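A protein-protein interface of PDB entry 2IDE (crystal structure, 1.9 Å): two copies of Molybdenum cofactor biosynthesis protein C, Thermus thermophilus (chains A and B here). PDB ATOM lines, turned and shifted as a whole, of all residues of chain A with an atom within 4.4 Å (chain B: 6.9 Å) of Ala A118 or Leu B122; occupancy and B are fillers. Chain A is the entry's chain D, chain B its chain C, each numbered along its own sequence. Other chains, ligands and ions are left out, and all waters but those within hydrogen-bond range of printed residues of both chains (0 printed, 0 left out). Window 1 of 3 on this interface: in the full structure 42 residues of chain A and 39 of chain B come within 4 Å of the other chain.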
ATOM      1  N   ILE A  71     -14.014  25.141  12.336  1.00  0.00           N
ATOM      2  CA  ILE A  71     -14.665  26.410  12.654  1.00  0.00           C
ATOM      3  C   ILE A  71     -14.715  26.530  14.173  1.00  0.00           C
ATOM      4  O   ILE A  71     -15.500  25.857  14.834  1.00  0.00           O
ATOM      5  CB  ILE A  71     -16.096  26.449  12.072  1.00  0.00           C
ATOM      6  CG1 ILE A  71     -16.083  25.943  10.621  1.00  0.00           C
ATOM      7  CG2 ILE A  71     -16.646  27.867  12.137  1.00  0.00           C
ATOM      8  CD1 ILE A  71     -15.133  26.697   9.698  1.00  0.00           C
ATOM      9  N   MET A 111     -22.820  25.443   8.494  1.00  0.00           N
ATOM     10  CA  MET A 111     -21.366  25.365   8.398  1.00  0.00           C
ATOM     11  C   MET A 111     -20.886  24.024   7.851  1.00  0.00           C
ATOM     12  O   MET A 111     -19.896  23.975   7.119  1.00  0.00           O
ATOM     13  CB  MET A 111     -20.707  25.648   9.753  1.00  0.00           C
ATOM     14  CG  MET A 111     -20.885  27.078  10.244  1.00  0.00           C
ATOM     15  SD  MET A 111     -20.564  28.328   8.962  1.00  0.00           S
ATOM     16  CE  MET A 111     -18.847  27.989   8.574  1.00  0.00           C
ATOM     17  N   MET A 114     -21.450  24.267   4.099  1.00  0.00           N
ATOM     18  CA  MET A 114     -20.486  25.189   3.509  1.00  0.00           C
ATOM     19  C   MET A 114     -19.078  24.598   3.517  1.00  0.00           C
ATOM     20  O   MET A 114     -18.353  24.696   2.526  1.00  0.00           O
ATOM     21  CB  MET A 114     -20.483  26.523   4.263  1.00  0.00           C
ATOM     22  CG  MET A 114     -21.732  27.388   4.038  1.00  0.00           C
ATOM     23  SD  MET A 114     -21.814  28.125   2.381  1.00  0.00           S
ATOM     24  CE  MET A 114     -20.689  29.483   2.564  1.00  0.00           C
ATOM     25  N   THR A 115     -18.700  23.985   4.635  1.00  0.00           N
ATOM     26  CA  THR A 115     -17.373  23.394   4.774  1.00  0.00           C
ATOM     27  C   THR A 115     -17.186  22.209   3.828  1.00  0.00           C
ATOM     28  O   THR A 115     -16.117  22.038   3.236  1.00  0.00           O
ATOM     29  CB  THR A 115     -17.124  22.963   6.234  1.00  0.00           C
ATOM     30  OG1 THR A 115     -17.254  24.108   7.089  1.00  0.00           O
ATOM     31  CG2 THR A 115     -15.717  22.373   6.393  1.00  0.00           C
ATOM     32  N   ALA A 116     -18.230  21.399   3.679  1.00  0.00           N
ATOM     33  CA  ALA A 116     -18.172  20.259   2.776  1.00  0.00           C
ATOM     34  C   ALA A 116     -17.839  20.750   1.364  1.00  0.00           C
ATOM     35  O   ALA A 116     -16.964  20.203   0.693  1.00  0.00           O
ATOM     36  CB  ALA A 116     -19.511  19.536   2.763  1.00  0.00           C
ATOM     37  N   CYS A 117     -18.543  21.786   0.915  1.00  0.00           N
ATOM     38  CA  CYS A 117     -18.315  22.317  -0.423  1.00  0.00           C
ATOM     39  C   CYS A 117     -16.946  22.964  -0.577  1.00  0.00           C
ATOM     40  O   CYS A 117     -16.289  22.774  -1.590  1.00  0.00           O
ATOM     41  CB  CYS A 117     -19.416  23.317  -0.790  1.00  0.00           C
ATOM     42  SG  CYS A 117     -21.040  22.544  -0.992  1.00  0.00           S
ATOM     43  N   ALA A 118     -16.515  23.719   0.431  1.00  0.00           N
ATOM     44  CA  ALA A 118     -15.214  24.385   0.381  1.00  0.00           C
ATOM     45  C   ALA A 118     -14.053  23.393   0.302  1.00  0.00           C
ATOM     46  O   ALA A 118     -13.119  23.574  -0.486  1.00  0.00           O
ATOM     47  CB  ALA A 118     -15.044  25.292   1.596  1.00  0.00           C
ATOM     48  N   VAL A 119     -14.103  22.343   1.113  1.00  0.00           N
ATOM     49  CA  VAL A 119     -13.027  21.360   1.100  1.00  0.00           C
ATOM     50  C   VAL A 119     -13.075  20.487  -0.164  1.00  0.00           C
ATOM     51  O   VAL A 119     -12.039  20.035  -0.648  1.00  0.00           O
ATOM     52  CB  VAL A 119     -13.056  20.495   2.384  1.00  0.00           C
ATOM     53  CG1 VAL A 119     -12.001  19.398   2.306  1.00  0.00           C
ATOM     54  CG2 VAL A 119     -12.792  21.384   3.593  1.00  0.00           C
ATOM     55  N   ALA A 120     -14.266  20.251  -0.704  1.00  0.00           N
ATOM     56  CA  ALA A 120     -14.358  19.480  -1.940  1.00  0.00           C
ATOM     57  C   ALA A 120     -13.717  20.330  -3.050  1.00  0.00           C
ATOM     58  O   ALA A 120     -12.977  19.822  -3.897  1.00  0.00           O
ATOM     59  CB  ALA A 120     -15.818  19.179  -2.282  1.00  0.00           C
ATOM     60  N   ALA A 121     -13.998  21.630  -3.033  1.00  0.00           N
ATOM     61  CA  ALA A 121     -13.443  22.536  -4.037  1.00  0.00           C
ATOM     62  C   ALA A 121     -11.914  22.541  -3.933  1.00  0.00           C
ATOM     63  O   ALA A 121     -11.213  22.421  -4.940  1.00  0.00           O
ATOM     64  CB  ALA A 121     -13.993  23.937  -3.836  1.00  0.00           C
ATOM     65  N   LEU A 122     -11.408  22.664  -2.708  1.00  0.00           N
ATOM     66  CA  LEU A 122      -9.965  22.668  -2.452  1.00  0.00           C
ATOM     67  C   LEU A 122      -9.322  21.367  -2.925  1.00  0.00           C
ATOM     68  O   LEU A 122      -8.165  21.348  -3.345  1.00  0.00           O
ATOM     69  CB  LEU A 122      -9.690  22.845  -0.955  1.00  0.00           C
ATOM     70  CG  LEU A 122      -9.935  24.220  -0.325  1.00  0.00           C
ATOM     71  CD1 LEU A 122      -9.927  24.094   1.205  1.00  0.00           C
ATOM     72  CD2 LEU A 122      -8.854  25.201  -0.801  1.00  0.00           C
ATOM     73  N   VAL B  32     -14.787  37.507   1.015  1.00  0.00           N
ATOM     74  CA  VAL B  32     -16.133  37.236   1.484  1.00  0.00           C
ATOM     75  C   VAL B  32     -16.948  38.473   1.123  1.00  0.00           C
ATOM     76  O   VAL B  32     -16.607  39.586   1.535  1.00  0.00           O
ATOM     77  CB  VAL B  32     -16.182  37.006   3.014  1.00  0.00           C
ATOM     78  CG1 VAL B  32     -17.615  36.718   3.445  1.00  0.00           C
ATOM     79  CG2 VAL B  32     -15.275  35.838   3.399  1.00  0.00           C
ATOM     80  N   ALA B  56     -11.550  34.528  12.674  1.00  0.00           N
ATOM     81  CA  ALA B  56     -11.268  33.970  11.351  1.00  0.00           C
ATOM     82  C   ALA B  56      -9.771  33.897  11.037  1.00  0.00           C
ATOM     83  O   ALA B  56      -9.302  32.936  10.422  1.00  0.00           O
ATOM     84  CB  ALA B  56     -11.990  34.786  10.273  1.00  0.00           C
ATOM     85  N   ILE B  71      -7.248  17.389   2.932  1.00  0.00           N
ATOM     86  CA  ILE B  71      -6.999  17.079   1.524  1.00  0.00           C
ATOM     87  C   ILE B  71      -6.392  15.671   1.483  1.00  0.00           C
ATOM     88  O   ILE B  71      -5.219  15.474   1.808  1.00  0.00           O
ATOM     89  CB  ILE B  71      -6.020  18.112   0.912  1.00  0.00           C
ATOM     90  CG1 ILE B  71      -6.479  19.531   1.265  1.00  0.00           C
ATOM     91  CG2 ILE B  71      -5.951  17.941  -0.604  1.00  0.00           C
ATOM     92  CD1 ILE B  71      -7.916  19.853   0.861  1.00  0.00           C
ATOM     93  N   ILE B  97      -8.856  38.141   2.620  1.00  0.00           N
ATOM     94  CA  ILE B  97      -8.043  37.231   3.406  1.00  0.00           C
ATOM     95  C   ILE B  97      -6.825  36.833   2.584  1.00  0.00           C
ATOM     96  O   ILE B  97      -6.933  36.547   1.391  1.00  0.00           O
ATOM     97  CB  ILE B  97      -8.834  35.965   3.770  1.00  0.00           C
ATOM     98  CG1 ILE B  97     -10.081  36.354   4.568  1.00  0.00           C
ATOM     99  CG2 ILE B  97      -7.954  35.014   4.571  1.00  0.00           C
ATOM    100  CD1 ILE B  97     -11.247  35.410   4.380  1.00  0.00           C
ATOM    101  N   THR B 115      -6.017  26.445   1.778  1.00  0.00           N
ATOM    102  CA  THR B 115      -6.894  25.979   2.848  1.00  0.00           C
ATOM    103  C   THR B 115      -7.036  27.008   3.970  1.00  0.00           C
ATOM    104  O   THR B 115      -8.132  27.227   4.490  1.00  0.00           O
ATOM    105  CB  THR B 115      -6.382  24.640   3.427  1.00  0.00           C
ATOM    106  OG1 THR B 115      -6.326  23.666   2.375  1.00  0.00           O
ATOM    107  CG2 THR B 115      -7.319  24.129   4.527  1.00  0.00           C
ATOM    108  N   ALA B 116      -5.927  27.637   4.345  1.00  0.00           N
ATOM    109  CA  ALA B 116      -5.956  28.645   5.395  1.00  0.00           C
ATOM    110  C   ALA B 116      -6.957  29.728   4.985  1.00  0.00           C
ATOM    111  O   ALA B 116      -7.792  30.160   5.781  1.00  0.00           O
ATOM    112  CB  ALA B 116      -4.561  29.249   5.580  1.00  0.00           C
ATOM    113  N   CYS B 117      -6.880  30.152   3.728  1.00  0.00           N
ATOM    114  CA  CYS B 117      -7.781  31.183   3.233  1.00  0.00           C
ATOM    115  C   CYS B 117      -9.236  30.736   3.209  1.00  0.00           C
ATOM    116  O   CYS B 117     -10.118  31.480   3.633  1.00  0.00           O
ATOM    117  CB  CYS B 117      -7.364  31.634   1.831  1.00  0.00           C
ATOM    118  SG  CYS B 117      -5.842  32.599   1.776  1.00  0.00           S
ATOM    119  N   ALA B 118      -9.489  29.529   2.708  1.00  0.00           N
ATOM    120  CA  ALA B 118     -10.852  29.022   2.626  1.00  0.00           C
ATOM    121  C   ALA B 118     -11.509  28.852   3.994  1.00  0.00           C
ATOM    122  O   ALA B 118     -12.686  29.170   4.157  1.00  0.00           O
ATOM    123  CB  ALA B 118     -10.873  27.698   1.870  1.00  0.00           C
ATOM    124  N   VAL B 119     -10.755  28.358   4.973  1.00  0.00           N
ATOM    125  CA  VAL B 119     -11.313  28.152   6.309  1.00  0.00           C
ATOM    126  C   VAL B 119     -11.496  29.469   7.054  1.00  0.00           C
ATOM    127  O   VAL B 119     -12.446  29.632   7.814  1.00  0.00           O
ATOM    128  CB  VAL B 119     -10.440  27.183   7.142  1.00  0.00           C
ATOM    129  CG1 VAL B 119     -11.037  27.013   8.546  1.00  0.00           C
ATOM    130  CG2 VAL B 119     -10.390  25.825   6.446  1.00  0.00           C
ATOM    131  N   ALA B 120     -10.589  30.412   6.833  1.00  0.00           N
ATOM    132  CA  ALA B 120     -10.711  31.720   7.460  1.00  0.00           C
ATOM    133  C   ALA B 120     -11.985  32.365   6.906  1.00  0.00           C
ATOM    134  O   ALA B 120     -12.745  33.007   7.636  1.00  0.00           O
ATOM    135  CB  ALA B 120      -9.502  32.570   7.122  1.00  0.00           C
ATOM    136  N   ALA B 121     -12.217  32.178   5.607  1.00  0.00           N
ATOM    137  CA  ALA B 121     -13.402  32.721   4.952  1.00  0.00           C
ATOM    138  C   ALA B 121     -14.657  32.059   5.513  1.00  0.00           C
ATOM    139  O   ALA B 121     -15.664  32.729   5.762  1.00  0.00           O
ATOM    140  CB  ALA B 121     -13.313  32.504   3.442  1.00  0.00           C
ATOM    141  N   LEU B 122     -14.596  30.744   5.706  1.00  0.00           N
ATOM    142  CA  LEU B 122     -15.727  30.009   6.261  1.00  0.00           C
ATOM    143  C   LEU B 122     -16.009  30.522   7.672  1.00  0.00           C
ATOM    144  O   LEU B 122     -17.163  30.606   8.087  1.00  0.00           O
ATOM    145  CB  LEU B 122     -15.425  28.501   6.310  1.00  0.00           C
ATOM    146  CG  LEU B 122     -15.409  27.734   4.980  1.00  0.00           C
ATOM    147  CD1 LEU B 122     -14.847  26.338   5.197  1.00  0.00           C
ATOM    148  CD2 LEU B 122     -16.827  27.648   4.405  1.00  0.00           C
ATOM    149  N   THR B 123     -14.954  30.877   8.403  1.00  0.00           N
ATOM    150  CA  THR B 123     -15.120  31.372   9.768  1.00  0.00           C
ATOM    151  C   THR B 123     -15.758  32.771   9.779  1.00  0.00           C
ATOM    152  O   THR B 123     -16.575  33.075  10.649  1.00  0.00           O
ATOM    153  CB  THR B 123     -13.763  31.358  10.517  1.00  0.00           C
ATOM    154  OG1 THR B 123     -13.264  30.013  10.546  1.00  0.00           O
ATOM    155  CG2 THR B 123     -13.919  31.839  11.955  1.00  0.00           C
ATOM    156  N   VAL B 124     -15.402  33.614   8.810  1.00  0.00           N
ATOM    157  CA  VAL B 124     -16.002  34.949   8.722  1.00  0.00           C
ATOM    158  C   VAL B 124     -17.501  34.740   8.532  1.00  0.00           C
ATOM    159  O   VAL B 124     -18.324  35.443   9.128  1.00  0.00           O
ATOM    160  CB  VAL B 124     -15.457  35.755   7.514  1.00  0.00           C
ATOM    161  CG1 VAL B 124     -16.247  37.058   7.350  1.00  0.00           C
ATOM    162  CG2 VAL B 124     -13.993  36.066   7.713  1.00  0.00           C
ATOM    163  N   TYR B 125     -17.846  33.763   7.697  1.00  0.00           N
ATOM    164  CA  TYR B 125     -19.236  33.427   7.419  1.00  0.00           C
ATOM    165  C   TYR B 125     -19.925  32.963   8.700  1.00  0.00           C
ATOM    166  O   TYR B 125     -21.033  33.394   9.012  1.00  0.00           O
ATOM    167  CB  TYR B 125     -19.317  32.315   6.365  1.00  0.00           C
ATOM    168  CG  TYR B 125     -20.735  31.916   6.013  1.00  0.00           C
ATOM    169  CD1 TYR B 125     -21.497  32.672   5.115  1.00  0.00           C
ATOM    170  CD2 TYR B 125     -21.331  30.805   6.606  1.00  0.00           C
ATOM    171  CE1 TYR B 125     -22.819  32.329   4.826  1.00  0.00           C
ATOM    172  CE2 TYR B 125     -22.649  30.454   6.325  1.00  0.00           C
ATOM    173  CZ  TYR B 125     -23.388  31.222   5.436  1.00  0.00           C
ATOM    174  OH  TYR B 125     -24.695  30.886   5.178  1.00  0.00           O
ATOM    175  N   ASP B 126     -19.264  32.078   9.439  1.00  0.00           N
ATOM    176  CA  ASP B 126     -19.821  31.564  10.689  1.00  0.00           C
ATOM    177  C   ASP B 126     -20.087  32.697  11.685  1.00  0.00           C
ATOM    178  O   ASP B 126     -21.108  32.697  12.372  1.00  0.00           O
ATOM    179  CB  ASP B 126     -18.851  30.558  11.321  1.00  0.00           C
ATOM    180  CG  ASP B 126     -19.400  29.932  12.592  1.00  0.00           C
ATOM    181  OD1 ASP B 126     -20.449  29.257  12.516  1.00  0.00           O
ATOM    182  OD2 ASP B 126     -18.779  30.108  13.663  1.00  0.00           O
ATOM    183  N   MET B 127     -19.168  33.657  11.735  1.00  0.00           N
ATOM    184  CA  MET B 127     -19.243  34.795  12.652  1.00  0.00           C
ATOM    185  C   MET B 127     -20.222  35.905  12.257  1.00  0.00           C
ATOM    186  O   MET B 127     -20.438  36.840  13.032  1.00  0.00           O
ATOM    187  CB  MET B 127     -17.851  35.415  12.826  1.00  0.00           C
ATOM    188  CG  MET B 127     -16.770  34.467  13.351  1.00  0.00           C
ATOM    189  SD  MET B 127     -17.067  33.840  15.026  1.00  0.00           S
ATOM    190  CE  MET B 127     -16.733  35.285  16.010  1.00  0.00           C
ATOM    191  N   ILE B 137     -18.669  33.396  -0.248  1.00  0.00           N
ATOM    192  CA  ILE B 137     -17.218  33.334  -0.224  1.00  0.00           C
ATOM    193  C   ILE B 137     -17.139  33.514  -1.730  1.00  0.00           C
ATOM    194  O   ILE B 137     -17.857  32.845  -2.472  1.00  0.00           O
ATOM    195  CB  ILE B 137     -16.653  31.975   0.266  1.00  0.00           C
ATOM    196  CG1 ILE B 137     -17.025  31.731   1.724  1.00  0.00           C
ATOM    197  CG2 ILE B 137     -15.135  31.965   0.067  1.00  0.00           C
ATOM    198  CD1 ILE B 137     -16.504  32.783   2.660  1.00  0.00           C
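The side-chain carboxylate (OD1) of Asp B126 sits close to the side-chain sulfur (SD) of Met A111 (3.7 Å).
OG1 of Thr B123 lies within hydrogen-bond range of O of Val B119.
The backbone carbonyl oxygen (O) of Met A111 is in hydrogen-bond range of the side-chain hydroxyl (OG1) of Thr A115 (2.6 Å).
Ile A71 touches Leu B122 (CD1 to CB, 3.8 Å).
Thr B123 touches Ile A71.
Ile A71 touches Asp B126 (CG2 to OD2, 3.4 Å).
Met A111 touches Leu B122.
SD of Met A111 touches CD2 of Tyr B125 (3.5 Å).
Leu B122 touches Met A114 (CD2 to O, 3.8 Å).
Met A114 touches Tyr B125 (CG to CE2, 3.9 Å).
Thr A115 touches Leu B122.
Ala A118 touches Leu B122 (CB to CD1, 3.8 Å).
Thr B115 touches Leu A122 (OG1 to CD1, 3.8 Å).
Of the printed residues of chain B, Met A114 touches Leu B122 and Tyr B125.
Cys A117 touches none of the printed residues of chain B.
Ala A118 touches just one residue of chain B: Leu B122.
Printed residues of chain B within 4 Å of Leu A122: Ile B71 (3.9 Å), Thr B115 (3.8 Å) and Ala B118 (3.8 Å).
Of the printed residues of chain A, Thr B115 touches Leu A122 (3.8 Å).
Of chain A, only Ile A71 (3.8 Å), Met A111 (3.1 Å), Met A114 (3.8 Å), Thr A115 (3.8 Å) and Ala A118 (3.8 Å) come within 4 Å of Leu B122.
Of the printed residues of chain A, Asp B126 touches Ile A71 (3.4 Å) and Met A111 (3.2 Å).
The nearest residue of chain B that does not touch Ala A118 is Ala B118 (4.8 Å).
Of the 18 printed residues of chain B, 7 touch a printed residue of chain A.
Hydrophobic or aromatic side chains of chain B that line the printed part of chain A: Ile B71, Ala B118, Leu B122 and Tyr B125.
Among the printed residues, no Asp or Glu carboxylate lies within 4 Å of a Lys or Arg side-chain nitrogen of the other chain.
Ile A71 touches Leu B122, and with the chains exchanged Leu A122 touches Ile B71.
Thr A115 touches Leu B122, and with the chains exchanged Leu A122 touches Thr B115.
Ala A118 touches Leu B122, and with the chains exchanged Leu A122 touches Ala B118.
9 positions are printed for both chains.
Of the 13 pairs that touch across the chains among the printed residues, 6 have their exchanged pair printed and touching as well.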
